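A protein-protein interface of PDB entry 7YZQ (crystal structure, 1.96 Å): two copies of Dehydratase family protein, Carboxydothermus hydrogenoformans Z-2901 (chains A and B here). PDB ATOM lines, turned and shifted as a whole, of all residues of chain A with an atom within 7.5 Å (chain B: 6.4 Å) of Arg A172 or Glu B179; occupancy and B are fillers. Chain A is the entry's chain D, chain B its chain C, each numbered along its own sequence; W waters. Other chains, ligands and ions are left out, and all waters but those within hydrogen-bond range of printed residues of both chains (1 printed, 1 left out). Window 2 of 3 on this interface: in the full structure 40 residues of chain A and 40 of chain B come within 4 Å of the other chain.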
ATOM      1  N   PRO A 166     -19.117  21.845 -23.199  1.00  0.00           N
ATOM      2  CA  PRO A 166     -20.188  20.841 -23.030  1.00  0.00           C
ATOM      3  C   PRO A 166     -19.728  19.729 -22.104  1.00  0.00           C
ATOM      4  O   PRO A 166     -18.553  19.655 -21.731  1.00  0.00           O
ATOM      5  CB  PRO A 166     -20.460  20.325 -24.463  1.00  0.00           C
ATOM      6  CG  PRO A 166     -19.218  20.670 -25.239  1.00  0.00           C
ATOM      7  CD  PRO A 166     -18.668  21.952 -24.608  1.00  0.00           C
ATOM      8  N   LYS A 168     -20.828  16.292 -22.782  1.00  0.00           N
ATOM      9  CA  LYS A 168     -20.790  15.095 -23.611  1.00  0.00           C
ATOM     10  C   LYS A 168     -20.073  15.455 -24.917  1.00  0.00           C
ATOM     11  O   LYS A 168     -19.646  16.589 -25.121  1.00  0.00           O
ATOM     12  CB  LYS A 168     -22.207  14.566 -23.877  1.00  0.00           C
ATOM     13  CG  LYS A 168     -22.941  14.070 -22.657  1.00  0.00           C
ATOM     14  CD  LYS A 168     -24.183  13.329 -23.079  1.00  0.00           C
ATOM     15  CE  LYS A 168     -25.316  13.430 -22.083  1.00  0.00           C
ATOM     16  NZ  LYS A 168     -26.609  12.762 -22.597  1.00  0.00           N
ATOM     17  N   LYS A 169     -19.936  14.486 -25.810  1.00  0.00           N
ATOM     18  CA  LYS A 169     -19.205  14.668 -27.064  1.00  0.00           C
ATOM     19  C   LYS A 169     -20.015  14.215 -28.282  1.00  0.00           C
ATOM     20  O   LYS A 169     -19.457  13.858 -29.331  1.00  0.00           O
ATOM     21  CB  LYS A 169     -17.871  13.933 -27.012  1.00  0.00           C
ATOM     22  CG  LYS A 169     -16.834  14.720 -26.278  1.00  0.00           C
ATOM     23  CD  LYS A 169     -15.681  13.911 -25.848  1.00  0.00           C
ATOM     24  CE  LYS A 169     -14.651  14.784 -25.113  1.00  0.00           C
ATOM     25  NZ  LYS A 169     -13.274  14.202 -25.374  1.00  0.00           N
ATOM     26  N   GLU A 170     -21.330  14.318 -28.200  1.00  0.00           N
ATOM     27  CA  GLU A 170     -22.197  14.030 -29.335  1.00  0.00           C
ATOM     28  C   GLU A 170     -22.267  15.233 -30.288  1.00  0.00           C
ATOM     29  O   GLU A 170     -21.644  16.292 -30.076  1.00  0.00           O
ATOM     30  CB  GLU A 170     -23.555  13.583 -28.807  1.00  0.00           C
ATOM     31  CG  GLU A 170     -23.403  12.417 -27.842  1.00  0.00           C
ATOM     32  CD  GLU A 170     -24.700  11.719 -27.497  1.00  0.00           C
ATOM     33  OE1 GLU A 170     -25.767  12.369 -27.537  1.00  0.00           O
ATOM     34  OE2 GLU A 170     -24.649  10.510 -27.165  1.00  0.00           O
ATOM     35  N   GLU A 171     -22.994  15.045 -31.395  1.00  0.00           N
ATOM     36  CA  GLU A 171     -22.975  16.053 -32.448  1.00  0.00           C
ATOM     37  C   GLU A 171     -23.407  17.415 -31.914  1.00  0.00           C
ATOM     38  O   GLU A 171     -22.773  18.436 -32.213  1.00  0.00           O
ATOM     39  CB  GLU A 171     -23.872  15.618 -33.609  1.00  0.00           C
ATOM     40  CG  GLU A 171     -23.950  16.602 -34.773  1.00  0.00           C
ATOM     41  CD  GLU A 171     -22.573  17.096 -35.248  1.00  0.00           C
ATOM     42  OE1 GLU A 171     -22.439  18.326 -35.472  1.00  0.00           O
ATOM     43  OE2 GLU A 171     -21.624  16.266 -35.395  1.00  0.00           O
ATOM     44  N   ARG A 172     -24.486  17.455 -31.128  1.00  0.00           N
ATOM     45  CA  ARG A 172     -24.941  18.729 -30.572  1.00  0.00           C
ATOM     46  C   ARG A 172     -23.872  19.363 -29.673  1.00  0.00           C
ATOM     47  O   ARG A 172     -23.748  20.589 -29.620  1.00  0.00           O
ATOM     48  CB  ARG A 172     -26.264  18.533 -29.809  1.00  0.00           C
ATOM     49  CG  ARG A 172     -27.499  18.581 -30.713  1.00  0.00           C
ATOM     50  CD  ARG A 172     -28.776  18.986 -29.943  1.00  0.00           C
ATOM     51  NE  ARG A 172     -28.895  18.283 -28.682  1.00  0.00           N
ATOM     52  CZ  ARG A 172     -29.648  17.198 -28.488  1.00  0.00           C
ATOM     53  NH1 ARG A 172     -30.385  16.684 -29.474  1.00  0.00           N
ATOM     54  NH2 ARG A 172     -29.695  16.634 -27.286  1.00  0.00           N
ATOM     55  N   ASP A 173     -23.127  18.543 -28.923  1.00  0.00           N
ATOM     56  CA  ASP A 173     -22.047  19.067 -28.090  1.00  0.00           C
ATOM     57  C   ASP A 173     -20.928  19.632 -28.955  1.00  0.00           C
ATOM     58  O   ASP A 173     -20.407  20.724 -28.689  1.00  0.00           O
ATOM     59  CB  ASP A 173     -21.496  17.969 -27.188  1.00  0.00           C
ATOM     60  CG  ASP A 173     -22.554  17.370 -26.262  1.00  0.00           C
ATOM     61  OD1 ASP A 173     -22.903  18.033 -25.275  1.00  0.00           O
ATOM     62  OD2 ASP A 173     -23.010  16.234 -26.509  1.00  0.00           O
ATOM     63  N   ARG A 174     -20.572  18.897 -30.013  1.00  0.00           N
ATOM     64  CA  ARG A 174     -19.516  19.342 -30.912  1.00  0.00           C
ATOM     65  C   ARG A 174     -19.876  20.676 -31.558  1.00  0.00           C
ATOM     66  O   ARG A 174     -19.034  21.570 -31.653  1.00  0.00           O
ATOM     67  CB  ARG A 174     -19.267  18.275 -31.977  1.00  0.00           C
ATOM     68  CG  ARG A 174     -18.587  17.014 -31.476  1.00  0.00           C
ATOM     69  CD  ARG A 174     -18.459  15.969 -32.625  1.00  0.00           C
ATOM     70  NE  ARG A 174     -18.854  14.639 -32.160  1.00  0.00           N
ATOM     71  CZ  ARG A 174     -19.677  13.813 -32.807  1.00  0.00           C
ATOM     72  NH1 ARG A 174     -19.966  12.640 -32.269  1.00  0.00           N
ATOM     73  NH2 ARG A 174     -20.207  14.151 -33.984  1.00  0.00           N
ATOM     74  N   LYS A 175     -21.128  20.835 -31.989  1.00  0.00           N
ATOM     75  CA  LYS A 175     -21.542  22.106 -32.580  1.00  0.00           C
ATOM     76  C   LYS A 175     -21.512  23.214 -31.535  1.00  0.00           C
ATOM     77  O   LYS A 175     -20.988  24.308 -31.786  1.00  0.00           O
ATOM     78  CB  LYS A 175     -22.933  21.946 -33.193  1.00  0.00           C
ATOM     79  CG  LYS A 175     -23.594  23.220 -33.577  1.00  0.00           C
ATOM     80  CD  LYS A 175     -22.932  23.813 -34.803  1.00  0.00           C
ATOM     81  CE  LYS A 175     -23.219  25.310 -34.898  1.00  0.00           C
ATOM     82  NZ  LYS A 175     -22.654  25.903 -36.155  1.00  0.00           N
ATOM     83  N   PHE A 176     -22.066  22.935 -30.350  1.00  0.00           N
ATOM     84  CA  PHE A 176     -21.994  23.864 -29.221  1.00  0.00           C
ATOM     85  C   PHE A 176     -20.571  24.351 -28.967  1.00  0.00           C
ATOM     86  O   PHE A 176     -20.321  25.552 -28.793  1.00  0.00           O
ATOM     87  CB  PHE A 176     -22.552  23.164 -27.979  1.00  0.00           C
ATOM     88  CG  PHE A 176     -22.834  24.077 -26.838  1.00  0.00           C
ATOM     89  CD1 PHE A 176     -21.882  24.320 -25.887  1.00  0.00           C
ATOM     90  CD2 PHE A 176     -24.064  24.673 -26.708  1.00  0.00           C
ATOM     91  CE1 PHE A 176     -22.144  25.170 -24.825  1.00  0.00           C
ATOM     92  CE2 PHE A 176     -24.327  25.526 -25.639  1.00  0.00           C
ATOM     93  CZ  PHE A 176     -23.369  25.762 -24.718  1.00  0.00           C
ATOM     94  N   TRP A 177     -19.623  23.436 -28.924  1.00  0.00           N
ATOM     95  CA  TRP A 177     -18.264  23.840 -28.596  1.00  0.00           C
ATOM     96  C   TRP A 177     -17.680  24.709 -29.701  1.00  0.00           C
ATOM     97  O   TRP A 177     -16.909  25.634 -29.412  1.00  0.00           O
ATOM     98  CB  TRP A 177     -17.397  22.609 -28.366  1.00  0.00           C
ATOM     99  CG  TRP A 177     -15.958  22.873 -27.961  1.00  0.00           C
ATOM    100  CD1 TRP A 177     -14.841  22.364 -28.551  1.00  0.00           C
ATOM    101  CD2 TRP A 177     -15.504  23.692 -26.884  1.00  0.00           C
ATOM    102  NE1 TRP A 177     -13.731  22.807 -27.910  1.00  0.00           N
ATOM    103  CE2 TRP A 177     -14.103  23.634 -26.885  1.00  0.00           C
ATOM    104  CE3 TRP A 177     -16.145  24.452 -25.909  1.00  0.00           C
ATOM    105  CZ2 TRP A 177     -13.327  24.280 -25.912  1.00  0.00           C
ATOM    106  CZ3 TRP A 177     -15.379  25.137 -24.990  1.00  0.00           C
ATOM    107  CH2 TRP A 177     -13.990  25.063 -25.007  1.00  0.00           C
ATOM    108  N   GLU A 178     -18.036  24.400 -30.962  1.00  0.00           N
ATOM    109  CA  GLU A 178     -17.641  25.217 -32.104  1.00  0.00           C
ATOM    110  C   GLU A 178     -18.108  26.646 -31.930  1.00  0.00           C
ATOM    111  O   GLU A 178     -17.360  27.589 -32.191  1.00  0.00           O
ATOM    112  CB  GLU A 178     -18.224  24.664 -33.407  1.00  0.00           C
ATOM    113  CG  GLU A 178     -17.532  23.430 -33.944  1.00  0.00           C
ATOM    114  CD  GLU A 178     -18.061  23.031 -35.332  1.00  0.00           C
ATOM    115  OE1 GLU A 178     -18.872  23.807 -35.918  1.00  0.00           O
ATOM    116  OE2 GLU A 178     -17.659  21.954 -35.815  1.00  0.00           O
ATOM    117  N   ARG B 174     -30.412  27.722 -23.803  1.00  0.00           N
ATOM    118  CA  ARG B 174     -31.847  27.445 -23.752  1.00  0.00           C
ATOM    119  C   ARG B 174     -32.284  26.558 -24.914  1.00  0.00           C
ATOM    120  O   ARG B 174     -33.204  25.736 -24.762  1.00  0.00           O
ATOM    121  CB  ARG B 174     -32.653  28.747 -23.776  1.00  0.00           C
ATOM    122  CG  ARG B 174     -32.440  29.586 -22.550  1.00  0.00           C
ATOM    123  CD  ARG B 174     -33.106  30.934 -22.649  1.00  0.00           C
ATOM    124  NE  ARG B 174     -32.883  31.632 -21.372  1.00  0.00           N
ATOM    125  CZ  ARG B 174     -33.515  31.367 -20.223  1.00  0.00           C
ATOM    126  NH1 ARG B 174     -34.453  30.418 -20.176  1.00  0.00           N
ATOM    127  NH2 ARG B 174     -33.205  32.060 -19.110  1.00  0.00           N
ATOM    128  N   LYS B 175     -31.664  26.741 -26.095  1.00  0.00           N
ATOM    129  CA  LYS B 175     -31.976  25.882 -27.236  1.00  0.00           C
ATOM    130  C   LYS B 175     -31.461  24.478 -26.985  1.00  0.00           C
ATOM    131  O   LYS B 175     -32.167  23.501 -27.227  1.00  0.00           O
ATOM    132  CB  LYS B 175     -31.384  26.454 -28.534  1.00  0.00           C
ATOM    133  CG  LYS B 175     -31.698  25.697 -29.782  1.00  0.00           C
ATOM    134  CD  LYS B 175     -31.052  26.400 -31.017  1.00  0.00           C
ATOM    135  CE  LYS B 175     -29.536  26.154 -31.095  1.00  0.00           C
ATOM    136  NZ  LYS B 175     -28.668  27.410 -30.875  1.00  0.00           N
ATOM    137  N   PHE B 176     -30.210  24.364 -26.518  1.00  0.00           N
ATOM    138  CA  PHE B 176     -29.631  23.067 -26.180  1.00  0.00           C
ATOM    139  C   PHE B 176     -30.559  22.295 -25.250  1.00  0.00           C
ATOM    140  O   PHE B 176     -30.818  21.110 -25.469  1.00  0.00           O
ATOM    141  CB  PHE B 176     -28.240  23.285 -25.547  1.00  0.00           C
ATOM    142  CG  PHE B 176     -27.414  22.041 -25.369  1.00  0.00           C
ATOM    143  CD1 PHE B 176     -27.662  21.168 -24.332  1.00  0.00           C
ATOM    144  CD2 PHE B 176     -26.363  21.760 -26.236  1.00  0.00           C
ATOM    145  CE1 PHE B 176     -26.886  20.028 -24.171  1.00  0.00           C
ATOM    146  CE2 PHE B 176     -25.602  20.638 -26.088  1.00  0.00           C
ATOM    147  CZ  PHE B 176     -25.848  19.766 -25.055  1.00  0.00           C
ATOM    148  N   TRP B 177     -31.069  22.957 -24.201  1.00  0.00           N
ATOM    149  CA  TRP B 177     -31.920  22.295 -23.212  1.00  0.00           C
ATOM    150  C   TRP B 177     -33.260  21.907 -23.818  1.00  0.00           C
ATOM    151  O   TRP B 177     -33.799  20.846 -23.512  1.00  0.00           O
ATOM    152  CB  TRP B 177     -32.111  23.222 -21.993  1.00  0.00           C
ATOM    153  CG  TRP B 177     -32.910  22.606 -20.875  1.00  0.00           C
ATOM    154  CD1 TRP B 177     -34.067  23.089 -20.302  1.00  0.00           C
ATOM    155  CD2 TRP B 177     -32.631  21.365 -20.217  1.00  0.00           C
ATOM    156  NE1 TRP B 177     -34.520  22.206 -19.341  1.00  0.00           N
ATOM    157  CE2 TRP B 177     -33.645  21.156 -19.255  1.00  0.00           C
ATOM    158  CE3 TRP B 177     -31.623  20.408 -20.351  1.00  0.00           C
ATOM    159  CZ2 TRP B 177     -33.692  20.009 -18.451  1.00  0.00           C
ATOM    160  CZ3 TRP B 177     -31.644  19.314 -19.524  1.00  0.00           C
ATOM    161  CH2 TRP B 177     -32.675  19.124 -18.579  1.00  0.00           C
ATOM    162  N   GLU B 178     -33.786  22.741 -24.707  1.00  0.00           N
ATOM    163  CA  GLU B 178     -34.977  22.401 -25.475  1.00  0.00           C
ATOM    164  C   GLU B 178     -34.800  21.090 -26.195  1.00  0.00           C
ATOM    165  O   GLU B 178     -35.653  20.217 -26.116  1.00  0.00           O
ATOM    166  CB  GLU B 178     -35.271  23.489 -26.507  1.00  0.00           C
ATOM    167  CG  GLU B 178     -36.681  23.955 -26.592  1.00  0.00           C
ATOM    168  CD  GLU B 178     -36.823  25.248 -27.429  1.00  0.00           C
ATOM    169  OE1 GLU B 178     -36.852  25.149 -28.682  1.00  0.00           O
ATOM    170  OE2 GLU B 178     -36.881  26.332 -26.803  1.00  0.00           O
ATOM    171  N   GLU B 179     -33.675  20.935 -26.888  1.00  0.00           N
ATOM    172  CA  GLU B 179     -33.421  19.706 -27.629  1.00  0.00           C
ATOM    173  C   GLU B 179     -33.277  18.521 -26.692  1.00  0.00           C
ATOM    174  O   GLU B 179     -33.713  17.404 -27.020  1.00  0.00           O
ATOM    175  CB  GLU B 179     -32.160  19.843 -28.491  1.00  0.00           C
ATOM    176  CG  GLU B 179     -32.296  20.832 -29.652  1.00  0.00           C
ATOM    177  CD  GLU B 179     -33.479  20.549 -30.529  1.00  0.00           C
ATOM    178  OE1 GLU B 179     -33.670  19.361 -30.923  1.00  0.00           O
ATOM    179  OE2 GLU B 179     -34.221  21.504 -30.831  1.00  0.00           O
ATOM    180  N   GLU B 180     -32.639  18.737 -25.531  1.00  0.00           N
ATOM    181  CA  GLU B 180     -32.535  17.658 -24.555  1.00  0.00           C
ATOM    182  C   GLU B 180     -33.911  17.216 -24.085  1.00  0.00           C
ATOM    183  O   GLU B 180     -34.167  16.012 -23.912  1.00  0.00           O
ATOM    184  CB  GLU B 180     -31.683  18.076 -23.351  1.00  0.00           C
ATOM    185  CG  GLU B 180     -30.215  18.118 -23.654  1.00  0.00           C
ATOM    186  CD  GLU B 180     -29.599  16.796 -23.850  1.00  0.00           C
ATOM    187  OE1 GLU B 180     -29.877  15.852 -23.068  1.00  0.00           O
ATOM    188  OE2 GLU B 180     -28.791  16.695 -24.798  1.00  0.00           O
ATOM    189  N   ILE B 181     -34.803  18.177 -23.848  1.00  0.00           N
ATOM    190  CA  ILE B 181     -36.164  17.857 -23.422  1.00  0.00           C
ATOM    191  C   ILE B 181     -36.919  17.059 -24.495  1.00  0.00           C
ATOM    192  O   ILE B 181     -37.704  16.150 -24.197  1.00  0.00           O
ATOM    193  CB  ILE B 181     -36.895  19.165 -23.076  1.00  0.00           C
ATOM    194  CG1 ILE B 181     -36.382  19.712 -21.724  1.00  0.00           C
ATOM    195  CG2 ILE B 181     -38.423  18.968 -23.102  1.00  0.00           C
ATOM    196  CD1 ILE B 181     -36.921  19.006 -20.521  1.00  0.00           C
ATOM    197  N   LYS B 182     -36.714  17.392 -25.758  1.00  0.00           N
ATOM    198  CA  LYS B 182     -37.391  16.645 -26.831  1.00  0.00           C
ATOM    199  C   LYS B 182     -36.809  15.242 -26.997  1.00  0.00           C
ATOM    200  O   LYS B 182     -37.549  14.283 -27.237  1.00  0.00           O
ATOM    201  CB  LYS B 182     -37.320  17.438 -28.146  1.00  0.00           C
ATOM    202  CG  LYS B 182     -38.113  18.735 -28.141  1.00  0.00           C
ATOM    203  CD  LYS B 182     -37.552  19.778 -29.099  1.00  0.00           C
ATOM    204  CE  LYS B 182     -37.380  19.210 -30.485  1.00  0.00           C
ATOM    205  NZ  LYS B 182     -37.125  20.311 -31.519  1.00  0.00           N
ATOM    206  N   ASP B 183     -35.495  15.100 -26.837  1.00  0.00           N
ATOM    207  CA  ASP B 183     -34.886  13.772 -26.828  1.00  0.00           C
ATOM    208  C   ASP B 183     -35.452  12.930 -25.689  1.00  0.00           C
ATOM    209  O   ASP B 183     -35.776  11.753 -25.878  1.00  0.00           O
ATOM    210  CB  ASP B 183     -33.367  13.869 -26.687  1.00  0.00           C
ATOM    211  CG  ASP B 183     -32.678  14.383 -27.943  1.00  0.00           C
ATOM    212  OD1 ASP B 183     -33.361  14.622 -28.962  1.00  0.00           O
ATOM    213  OD2 ASP B 183     -31.434  14.507 -27.904  1.00  0.00           O
ATOM    214  N   PHE B 184     -35.598  13.527 -24.499  1.00  0.00           N
ATOM    215  CA  PHE B 184     -36.148  12.791 -23.356  1.00  0.00           C
ATOM    216  C   PHE B 184     -37.597  12.382 -23.621  1.00  0.00           C
ATOM    217  O   PHE B 184     -38.003  11.252 -23.326  1.00  0.00           O
ATOM    218  CB  PHE B 184     -36.047  13.646 -22.083  1.00  0.00           C
ATOM    219  CG  PHE B 184     -36.571  12.964 -20.847  1.00  0.00           C
ATOM    220  CD1 PHE B 184     -35.983  11.802 -20.391  1.00  0.00           C
ATOM    221  CD2 PHE B 184     -37.656  13.447 -20.195  1.00  0.00           C
ATOM    222  CE1 PHE B 184     -36.457  11.145 -19.314  1.00  0.00           C
ATOM    223  CE2 PHE B 184     -38.132  12.803 -19.035  1.00  0.00           C
ATOM    224  CZ  PHE B 184     -37.546  11.657 -18.618  1.00  0.00           C
ATOM    225  N   ALA B 333     -39.446  23.022 -20.975  1.00  0.00           N
ATOM    226  CA  ALA B 333     -38.018  23.314 -20.857  1.00  0.00           C
ATOM    227  C   ALA B 333     -37.794  24.666 -20.190  1.00  0.00           C
ATOM    228  O   ALA B 333     -36.951  24.798 -19.288  1.00  0.00           O
ATOM    229  CB  ALA B 333     -37.316  23.299 -22.221  1.00  0.00           C
HETATM  230  O   HOH W   1     -27.877  14.111 -24.165  1.00  0.00           O
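Phe A176 touches its own counterpart, Phe B176. Positions printed for both chains: 174, 175, 176, 177 and 178. Of the 6 pairs that touch across the chains among the printed residues, 1 has its exchanged pair printed and touching as well.
The side-chain carboxylate (OE2) of Glu B180 lies within salt-bridge range of the guanidinium group (NH2) of Arg A172 (2.6 Å). The side-chain carboxylate of Asp B183 is in salt-bridge range of the guanidinium group of Arg A172, at 2.8 Å.
Water W1 lies within hydrogen-bond range of NZ of Lys A168 (2.4 Å) and OE2 of Glu B180 (2.8 Å).
O of Arg A172 touches CE2 of Phe B176 (3.99 Å). CB of Glu B179 touches NE of Arg A172, 3.6 Å away. Phe B176 touches Asp A173. Phe B176 touches Phe A176.
The side-chain carboxylate (OE2) of Glu B179 lies within salt-bridge range of the side-chain amino group (NZ) of Lys B182, 3.2 Å away. The backbone NH (N) of Glu A170 is in hydrogen-bond range of the side-chain carboxylate (OD2) of Asp A173 (3.1 Å).
Of the 12 printed residues of chain B, 4 touch a printed residue of chain A. Hydrophobic or aromatic side chains of chain B that line the printed part of chain A: Phe B176. Hydrophobic or aromatic side chains of chain A that line the printed part of chain B: Phe A176. Among the printed residues, 6 pairs touch across the chains.
Of the printed residues of chain B, Arg A172 touches Phe B176, Glu B179, Glu B180 and Asp B183. Of chain A, only Arg A172 comes within 4 Å of Glu B179. Printed residues of chain B within 4 Å of Phe A176: Phe B176 (3.7 Å). Printed residues of chain B within 4 Å of Asp A173: Phe B176. Of the printed residues of chain A, Phe B176 touches Arg A172, Asp A173 and Phe A176. Printed residues of chain A within 4 Å of Asp B183: Arg A172. Of the printed residues of chain A, Glu B180 touches Arg A172 (2.6 Å). Trp B177 touches none of the printed residues of chain A. Lys A169 touches none of the printed residues of chain B. The nearest printed residue of chain B that does not touch Arg A172 is Lys B175 (6.3 Å). The nearest printed residue of chain A that does not touch Glu B179 is Asp A173 (9.1 Å).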
